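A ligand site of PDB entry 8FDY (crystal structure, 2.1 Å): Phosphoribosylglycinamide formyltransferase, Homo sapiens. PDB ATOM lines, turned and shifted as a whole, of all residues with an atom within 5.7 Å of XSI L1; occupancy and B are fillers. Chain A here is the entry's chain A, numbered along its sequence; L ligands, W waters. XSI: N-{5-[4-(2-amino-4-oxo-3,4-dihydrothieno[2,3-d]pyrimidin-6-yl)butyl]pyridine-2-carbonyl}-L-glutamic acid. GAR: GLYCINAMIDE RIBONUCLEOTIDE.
The backbone carbonyl oxygen of Lys 117 is in hydrogen-bond range of the side-chain amide nitrogen of Gln 124, 2.8 Å away.
The backbone NH (N) of Asn 107 sits at hydrogen-bond distance from the backbone carbonyl oxygen (O) of His 138, at 2.9 Å.
OD2 of Asp 145 sits at hydrogen-bond distance from N of Gly 118 (2.8 Å).
The backbone carbonyl oxygen (O) of Arg 91 sits close to a sulfur (S07) of XSI L1, 3.0 Å away.
The backbone carbonyl oxygen (O) of Lys 117 lies close to an oxygen (O24) of XSI L1.
Residues that only touch XSI L1: Phe 89, Val 144, Asn 107, Val 98, Val 140, Gly 118, Met 90, Gln 124, Glu 142 and Ile 92.
Hydrophobic or aromatic side chains that line XSI L1: Met 90, Ile 92, Leu 93, Val 98, Val 140 and Val 144.
16 residues have an atom within 4 Å of XSI L1: Phe 89, Met 90, Arg 91, Ile 92, Leu 93, Val 98, Asn 107, Lys 117, Gly 118, Ser 119, Gln 124, Val 140, Ala 141, Glu 142, Val 144 and Asp 145.
Along chain A the residues within 4 Å of XSI L1 span positions 89 to 145.
O of Ala 141 sits at hydrogen-bond distance from N03 of XSI L1 (3.0 Å).
O10 of XSI L1 sits at hydrogen-bond distance from N of Asp 145, 3.0 Å away.
The backbone carbonyl oxygen (O) of Leu 93 sits at hydrogen-bond distance from a nitrogen (N11) of XSI L1.
OG of Ser 119 is in hydrogen-bond range of N19 of XSI L1, at 3.1 Å.
N01 of XSI L1 lies within hydrogen-bond range of N of Leu 93, at 3.2 Å.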
ATOM      1  N   LEU A  86     -15.466  -1.433  30.743  1.00  0.00           N
ATOM      2  CA  LEU A  86     -14.472  -2.287  31.376  1.00  0.00           C
ATOM      3  C   LEU A  86     -14.078  -1.631  32.691  1.00  0.00           C
ATOM      4  O   LEU A  86     -13.502  -0.546  32.699  1.00  0.00           O
ATOM      5  CB  LEU A  86     -13.265  -2.471  30.469  1.00  0.00           C
ATOM      6  CG  LEU A  86     -13.576  -2.932  29.036  1.00  0.00           C
ATOM      7  CD1 LEU A  86     -12.284  -3.274  28.305  1.00  0.00           C
ATOM      8  CD2 LEU A  86     -14.504  -4.126  29.053  1.00  0.00           C
ATOM      9  N   PHE A  89     -11.416  -4.853  34.468  1.00  0.00           N
ATOM     10  CA  PHE A  89     -11.437  -6.103  33.717  1.00  0.00           C
ATOM     11  C   PHE A  89     -10.013  -6.376  33.220  1.00  0.00           C
ATOM     12  O   PHE A  89      -9.464  -5.586  32.449  1.00  0.00           O
ATOM     13  CB  PHE A  89     -12.427  -5.975  32.560  1.00  0.00           C
ATOM     14  CG  PHE A  89     -12.599  -7.230  31.762  1.00  0.00           C
ATOM     15  CD1 PHE A  89     -13.337  -8.292  32.256  1.00  0.00           C
ATOM     16  CD2 PHE A  89     -12.052  -7.333  30.487  1.00  0.00           C
ATOM     17  CE1 PHE A  89     -13.505  -9.443  31.501  1.00  0.00           C
ATOM     18  CE2 PHE A  89     -12.220  -8.484  29.732  1.00  0.00           C
ATOM     19  CZ  PHE A  89     -12.941  -9.529  30.244  1.00  0.00           C
ATOM     20  N   MET A  90      -9.432  -7.484  33.668  1.00  0.00           N
ATOM     21  CA  MET A  90      -8.001  -7.751  33.468  1.00  0.00           C
ATOM     22  C   MET A  90      -7.750  -8.867  32.467  1.00  0.00           C
ATOM     23  O   MET A  90      -6.880  -9.716  32.665  1.00  0.00           O
ATOM     24  CB  MET A  90      -7.317  -8.073  34.801  1.00  0.00           C
ATOM     25  CG  MET A  90      -7.322  -6.930  35.814  1.00  0.00           C
ATOM     26  SD  MET A  90      -6.507  -5.425  35.244  1.00  0.00           S
ATOM     27  CE  MET A  90      -7.189  -4.223  36.375  1.00  0.00           C
ATOM     28  N   ARG A  91      -8.516  -8.901  31.377  1.00  0.00           N
ATOM     29  CA  ARG A  91      -8.163  -9.687  30.216  1.00  0.00           C
ATOM     30  C   ARG A  91      -8.037  -8.751  29.027  1.00  0.00           C
ATOM     31  O   ARG A  91      -8.562  -7.632  29.025  1.00  0.00           O
ATOM     32  CB  ARG A  91      -9.207 -10.784  29.915  1.00  0.00           C
ATOM     33  CG  ARG A  91      -9.230 -11.914  30.938  1.00  0.00           C
ATOM     34  CD  ARG A  91      -9.400 -13.284  30.264  1.00  0.00           C
ATOM     35  NE  ARG A  91      -9.725 -14.341  31.233  1.00  0.00           N
ATOM     36  CZ  ARG A  91      -8.858 -15.245  31.689  1.00  0.00           C
ATOM     37  NH1 ARG A  91      -7.605 -15.237  31.268  1.00  0.00           N
ATOM     38  NH2 ARG A  91      -9.259 -16.150  32.567  1.00  0.00           N
ATOM     39  N   ILE A  92      -7.306  -9.184  28.018  1.00  0.00           N
ATOM     40  CA  ILE A  92      -7.169  -8.429  26.789  1.00  0.00           C
ATOM     41  C   ILE A  92      -8.206  -8.953  25.806  1.00  0.00           C
ATOM     42  O   ILE A  92      -8.399 -10.172  25.679  1.00  0.00           O
ATOM     43  CB  ILE A  92      -5.741  -8.522  26.223  1.00  0.00           C
ATOM     44  CG1 ILE A  92      -4.758  -7.880  27.197  1.00  0.00           C
ATOM     45  CG2 ILE A  92      -5.653  -7.824  24.883  1.00  0.00           C
ATOM     46  CD1 ILE A  92      -3.381  -7.700  26.627  1.00  0.00           C
ATOM     47  N   LEU A  93      -8.892  -8.035  25.129  1.00  0.00           N
ATOM     48  CA  LEU A  93      -9.965  -8.402  24.227  1.00  0.00           C
ATOM     49  C   LEU A  93      -9.439  -8.587  22.808  1.00  0.00           C
ATOM     50  O   LEU A  93      -8.466  -7.954  22.408  1.00  0.00           O
ATOM     51  CB  LEU A  93     -11.056  -7.330  24.253  1.00  0.00           C
ATOM     52  CG  LEU A  93     -11.588  -7.073  25.660  1.00  0.00           C
ATOM     53  CD1 LEU A  93     -12.461  -5.829  25.688  1.00  0.00           C
ATOM     54  CD2 LEU A  93     -12.364  -8.291  26.137  1.00  0.00           C
ATOM     55  N   SER A  94     -10.098  -9.476  22.074  1.00  0.00           N
ATOM     56  CA  SER A  94      -9.683  -9.776  20.714  1.00  0.00           C
ATOM     57  C   SER A  94     -10.006  -8.611  19.772  1.00  0.00           C
ATOM     58  O   SER A  94     -10.833  -7.741  20.063  1.00  0.00           O
ATOM     59  CB  SER A  94     -10.372 -11.046  20.226  1.00  0.00           C
ATOM     60  OG  SER A  94     -11.782 -10.910  20.285  1.00  0.00           O
ATOM     61  N   VAL A  98     -13.189  -6.076  19.785  1.00  0.00           N
ATOM     62  CA  VAL A  98     -12.968  -4.651  19.913  1.00  0.00           C
ATOM     63  C   VAL A  98     -13.488  -3.919  18.676  1.00  0.00           C
ATOM     64  O   VAL A  98     -14.094  -2.855  18.782  1.00  0.00           O
ATOM     65  CB  VAL A  98     -11.479  -4.336  20.162  1.00  0.00           C
ATOM     66  CG1 VAL A  98     -11.275  -2.843  20.258  1.00  0.00           C
ATOM     67  CG2 VAL A  98     -11.023  -5.002  21.448  1.00  0.00           C
ATOM     68  N   ASN A 107     -13.065   2.211  28.861  1.00  0.00           N
ATOM     69  CA  ASN A 107     -12.157   1.629  29.834  1.00  0.00           C
ATOM     70  C   ASN A 107     -11.607   2.731  30.718  1.00  0.00           C
ATOM     71  O   ASN A 107     -11.424   3.868  30.282  1.00  0.00           O
ATOM     72  CB  ASN A 107     -11.027   0.881  29.141  1.00  0.00           C
ATOM     73  CG  ASN A 107     -10.014   0.344  30.106  1.00  0.00           C
ATOM     74  OD1 ASN A 107     -10.345  -0.462  30.969  1.00  0.00           O
ATOM     75  ND2 ASN A 107      -8.775   0.805  29.978  1.00  0.00           N
ATOM     76  N   LYS A 117       1.158   3.326  29.738  1.00  0.00           N
ATOM     77  CA  LYS A 117       0.252   2.311  29.221  1.00  0.00           C
ATOM     78  C   LYS A 117       0.623   0.962  29.816  1.00  0.00           C
ATOM     79  O   LYS A 117       1.759   0.709  30.205  1.00  0.00           O
ATOM     80  CB  LYS A 117       0.331   2.263  27.703  1.00  0.00           C
ATOM     81  CG  LYS A 117      -0.045   3.573  27.072  1.00  0.00           C
ATOM     82  CD  LYS A 117       0.391   3.600  25.622  1.00  0.00           C
ATOM     83  CE  LYS A 117      -0.224   4.778  24.897  1.00  0.00           C
ATOM     84  NZ  LYS A 117       0.060   4.695  23.435  1.00  0.00           N
ATOM     85  N   GLY A 118      -0.361   0.080  29.887  1.00  0.00           N
ATOM     86  CA  GLY A 118      -0.097  -1.272  30.328  1.00  0.00           C
ATOM     87  C   GLY A 118      -0.467  -1.502  31.779  1.00  0.00           C
ATOM     88  O   GLY A 118      -1.111  -0.700  32.448  1.00  0.00           O
ATOM     89  N   SER A 119      -0.004  -2.644  32.279  1.00  0.00           N
ATOM     90  CA  SER A 119      -0.657  -3.286  33.407  1.00  0.00           C
ATOM     91  C   SER A 119      -0.261  -2.706  34.763  1.00  0.00           C
ATOM     92  O   SER A 119      -1.057  -2.765  35.698  1.00  0.00           O
ATOM     93  CB  SER A 119      -0.353  -4.781  33.386  1.00  0.00           C
ATOM     94  OG  SER A 119       1.033  -4.980  33.191  1.00  0.00           O
ATOM     95  N   ASN A 120       0.944  -2.158  34.912  1.00  0.00           N
ATOM     96  CA  ASN A 120       1.314  -1.723  36.257  1.00  0.00           C
ATOM     97  C   ASN A 120       1.505  -0.204  36.318  1.00  0.00           C
ATOM     98  O   ASN A 120       2.588   0.269  36.672  1.00  0.00           O
ATOM     99  CB  ASN A 120       2.577  -2.444  36.712  1.00  0.00           C
ATOM    100  CG  ASN A 120       2.335  -3.909  37.013  1.00  0.00           C
ATOM    101  OD1 ASN A 120       2.861  -4.790  36.327  1.00  0.00           O
ATOM    102  ND2 ASN A 120       1.543  -4.190  38.037  1.00  0.00           N
ATOM    103  N   GLN A 124       4.850   1.972  37.334  1.00  0.00           N
ATOM    104  CA  GLN A 124       5.524   2.785  36.324  1.00  0.00           C
ATOM    105  C   GLN A 124       5.624   4.239  36.771  1.00  0.00           C
ATOM    106  O   GLN A 124       6.692   4.842  36.729  1.00  0.00           O
ATOM    107  CB  GLN A 124       4.775   2.700  34.997  1.00  0.00           C
ATOM    108  CG  GLN A 124       4.601   1.302  34.428  1.00  0.00           C
ATOM    109  CD  GLN A 124       4.042   1.357  33.021  1.00  0.00           C
ATOM    110  OE1 GLN A 124       4.580   2.058  32.150  1.00  0.00           O
ATOM    111  NE2 GLN A 124       2.949   0.640  32.776  1.00  0.00           N
ATOM    112  N   HIS A 138     -11.215   6.125  28.352  1.00  0.00           N
ATOM    113  CA  HIS A 138     -10.986   6.172  26.925  1.00  0.00           C
ATOM    114  C   HIS A 138     -11.835   5.116  26.234  1.00  0.00           C
ATOM    115  O   HIS A 138     -12.245   4.123  26.847  1.00  0.00           O
ATOM    116  CB  HIS A 138      -9.506   5.972  26.580  1.00  0.00           C
ATOM    117  CG  HIS A 138      -8.944   4.646  27.030  1.00  0.00           C
ATOM    118  ND1 HIS A 138      -8.840   3.565  26.183  1.00  0.00           N
ATOM    119  CD2 HIS A 138      -8.453   4.245  28.220  1.00  0.00           C
ATOM    120  CE1 HIS A 138      -8.321   2.543  26.850  1.00  0.00           C
ATOM    121  NE2 HIS A 138      -8.068   2.929  28.090  1.00  0.00           N
ATOM    122  N   VAL A 140     -12.008   1.976  23.836  1.00  0.00           N
ATOM    123  CA  VAL A 140     -11.080   0.874  23.670  1.00  0.00           C
ATOM    124  C   VAL A 140     -10.783   0.704  22.182  1.00  0.00           C
ATOM    125  O   VAL A 140     -11.698   0.529  21.381  1.00  0.00           O
ATOM    126  CB  VAL A 140     -11.625  -0.416  24.291  1.00  0.00           C
ATOM    127  CG1 VAL A 140     -10.700  -1.579  23.944  1.00  0.00           C
ATOM    128  CG2 VAL A 140     -11.729  -0.249  25.787  1.00  0.00           C
ATOM    129  N   ALA A 141      -9.510   0.763  21.827  1.00  0.00           N
ATOM    130  CA  ALA A 141      -9.041   0.478  20.480  1.00  0.00           C
ATOM    131  C   ALA A 141      -8.237  -0.826  20.480  1.00  0.00           C
ATOM    132  O   ALA A 141      -8.082  -1.491  21.511  1.00  0.00           O
ATOM    133  CB  ALA A 141      -8.201   1.645  19.944  1.00  0.00           C
ATOM    134  N   GLU A 142      -7.726  -1.195  19.301  1.00  0.00           N
ATOM    135  CA  GLU A 142      -7.017  -2.464  19.191  1.00  0.00           C
ATOM    136  C   GLU A 142      -5.657  -2.404  19.880  1.00  0.00           C
ATOM    137  O   GLU A 142      -5.219  -3.385  20.480  1.00  0.00           O
ATOM    138  CB  GLU A 142      -6.871  -2.859  17.721  1.00  0.00           C
ATOM    139  CG  GLU A 142      -8.202  -2.961  16.966  1.00  0.00           C
ATOM    140  CD  GLU A 142      -8.837  -1.599  16.741  1.00  0.00           C
ATOM    141  OE1 GLU A 142      -8.260  -0.584  17.205  1.00  0.00           O
ATOM    142  OE2 GLU A 142      -9.917  -1.534  16.107  1.00  0.00           O
ATOM    143  N   ASP A 143      -4.982  -1.246  19.799  1.00  0.00           N
ATOM    144  CA  ASP A 143      -3.759  -1.029  20.577  1.00  0.00           C
ATOM    145  C   ASP A 143      -4.141  -0.738  22.014  1.00  0.00           C
ATOM    146  O   ASP A 143      -4.776   0.278  22.306  1.00  0.00           O
ATOM    147  CB  ASP A 143      -2.959   0.128  19.977  1.00  0.00           C
ATOM    148  CG  ASP A 143      -2.307  -0.231  18.665  1.00  0.00           C
ATOM    149  OD1 ASP A 143      -1.295  -0.966  18.679  1.00  0.00           O
ATOM    150  OD2 ASP A 143      -2.829   0.197  17.619  1.00  0.00           O
ATOM    151  N   VAL A 144      -3.751  -1.632  22.930  1.00  0.00           N
ATOM    152  CA  VAL A 144      -4.105  -1.489  24.336  1.00  0.00           C
ATOM    153  C   VAL A 144      -3.790  -0.078  24.813  1.00  0.00           C
ATOM    154  O   VAL A 144      -2.681   0.429  24.609  1.00  0.00           O
ATOM    155  CB  VAL A 144      -3.368  -2.566  25.177  1.00  0.00           C
ATOM    156  CG1 VAL A 144      -3.732  -2.421  26.646  1.00  0.00           C
ATOM    157  CG2 VAL A 144      -3.718  -3.956  24.667  1.00  0.00           C
ATOM    158  N   ASP A 145      -4.790   0.557  25.438  1.00  0.00           N
ATOM    159  CA  ASP A 145      -4.657   1.917  25.977  1.00  0.00           C
ATOM    160  C   ASP A 145      -4.297   2.932  24.896  1.00  0.00           C
ATOM    161  O   ASP A 145      -3.542   3.876  25.128  1.00  0.00           O
ATOM    162  CB  ASP A 145      -3.642   1.980  27.119  1.00  0.00           C
ATOM    163  CG  ASP A 145      -3.907   0.965  28.185  1.00  0.00           C
ATOM    164  OD1 ASP A 145      -5.096   0.716  28.501  1.00  0.00           O
ATOM    165  OD2 ASP A 145      -2.928   0.398  28.706  1.00  0.00           O
ATOM    166  N   ALA A 146      -4.849   2.735  23.690  1.00  0.00           N
ATOM    167  CA  ALA A 146      -4.525   3.608  22.568  1.00  0.00           C
ATOM    168  C   ALA A 146      -5.770   4.143  21.873  1.00  0.00           C
ATOM    169  O   ALA A 146      -5.660   4.670  20.759  1.00  0.00           O
ATOM    170  CB  ALA A 146      -3.639   2.876  21.560  1.00  0.00           C
HETATM  171  C12 XSI L   1      -1.995  -4.899  30.003  1.00  0.00           C
HETATM  172  C14 XSI L   1      -2.999  -3.956  29.815  1.00  0.00           C
HETATM  173  C15 XSI L   1      -3.469  -6.219  31.260  1.00  0.00           C
HETATM  174  C16 XSI L   1      -4.219  -4.164  30.362  1.00  0.00           C
HETATM  175  C21 XSI L   1       2.475  -3.640  30.138  1.00  0.00           C
HETATM  176  C22 XSI L   1       2.990  -2.714  29.043  1.00  0.00           C
HETATM  177  C17 XSI L   1      -0.610  -4.693  29.406  1.00  0.00           C
HETATM  178  C23 XSI L   1       4.035  -1.745  29.590  1.00  0.00           C
HETATM  179  N11 XSI L   1      -7.885  -4.915  22.793  1.00  0.00           N
HETATM  180  N13 XSI L   1      -2.256  -6.015  30.719  1.00  0.00           N
HETATM  181  C20 XSI L   1       1.898  -4.943  29.595  1.00  0.00           C
HETATM  182  C02 XSI L   1      -7.884  -4.215  24.055  1.00  0.00           C
HETATM  183  C04 XSI L   1      -7.555  -2.258  25.228  1.00  0.00           C
HETATM  184  C05 XSI L   1      -7.919  -2.395  27.714  1.00  0.00           C
HETATM  185  C06 XSI L   1      -8.280  -3.326  28.686  1.00  0.00           C
HETATM  186  C08 XSI L   1      -7.867  -2.914  26.396  1.00  0.00           C
HETATM  187  C09 XSI L   1      -8.194  -4.279  26.312  1.00  0.00           C
HETATM  188  C26 XSI L   1       2.789  -6.132  29.952  1.00  0.00           C
HETATM  189  C29 XSI L   1      -8.409  -3.062  30.180  1.00  0.00           C
HETATM  190  C30 XSI L   1      -7.122  -3.508  30.867  1.00  0.00           C
HETATM  191  C31 XSI L   1      -6.960  -5.028  30.798  1.00  0.00           C
HETATM  192  C32 XSI L   1      -5.840  -5.535  31.692  1.00  0.00           C
HETATM  193  C33 XSI L   1      -4.464  -5.288  31.076  1.00  0.00           C
HETATM  194  N01 XSI L   1      -8.190  -4.894  25.156  1.00  0.00           N
HETATM  195  N03 XSI L   1      -7.562  -2.924  24.078  1.00  0.00           N
HETATM  196  N19 XSI L   1       0.567  -5.130  30.150  1.00  0.00           N
HETATM  197  O10 XSI L   1      -7.275  -1.111  25.256  1.00  0.00           O
HETATM  198  O18 XSI L   1      -0.490  -4.198  28.340  1.00  0.00           O
HETATM  199  O24 XSI L   1       4.334  -0.694  28.955  1.00  0.00           O
HETATM  200  O25 XSI L   1       4.595  -1.998  30.685  1.00  0.00           O
HETATM  201  O27 XSI L   1       2.281  -7.196  30.395  1.00  0.00           O
HETATM  202  O28 XSI L   1       4.045  -6.064  29.806  1.00  0.00           O
HETATM  203  S07 XSI L   1      -8.530  -4.802  27.898  1.00  0.00           S
HETATM  204  C1  GAR L   2      -8.782   0.274  38.634  1.00  0.00           C
HETATM  205  O6  GAR L   2      -8.114   1.094  39.611  1.00  0.00           O
HETATM  206  C2  GAR L   2      -8.212   0.516  37.231  1.00  0.00           C
HETATM  207  O8  GAR L   2      -7.540   1.769  37.252  1.00  0.00           O
HETATM  208  C3  GAR L   2      -7.328  -0.700  36.957  1.00  0.00           C
HETATM  209  O4  GAR L   2      -7.827  -1.740  37.824  1.00  0.00           O
HETATM  210  C5  GAR L   2      -8.559  -1.195  38.951  1.00  0.00           C
HETATM  211  C10 GAR L   2      -9.878  -1.908  39.273  1.00  0.00           C
HETATM  212  O12 GAR L   2     -10.401  -1.359  40.492  1.00  0.00           O
HETATM  213  N19 GAR L   2      -7.333  -1.198  35.573  1.00  0.00           N
HETATM  214  C21 GAR L   2      -6.182  -1.297  34.893  1.00  0.00           C
HETATM  215  O22 GAR L   2      -5.071  -1.146  35.391  1.00  0.00           O
HETATM  216  C23 GAR L   2      -6.286  -1.639  33.427  1.00  0.00           C
HETATM  217  N24 GAR L   2      -6.236  -0.496  32.507  1.00  0.00           N
HETATM  218  P15 GAR L   2     -11.932  -1.625  40.951  1.00  0.00           P
HETATM  219  O16 GAR L   2     -12.785  -0.900  39.934  1.00  0.00           O
HETATM  220  O17 GAR L   2     -12.066  -3.132  40.885  1.00  0.00           O
HETATM  221  O18 GAR L   2     -11.988  -1.028  42.338  1.00  0.00           O
HETATM  222  O   HOH W   1      -7.365   0.957  23.704  1.00  0.00           O
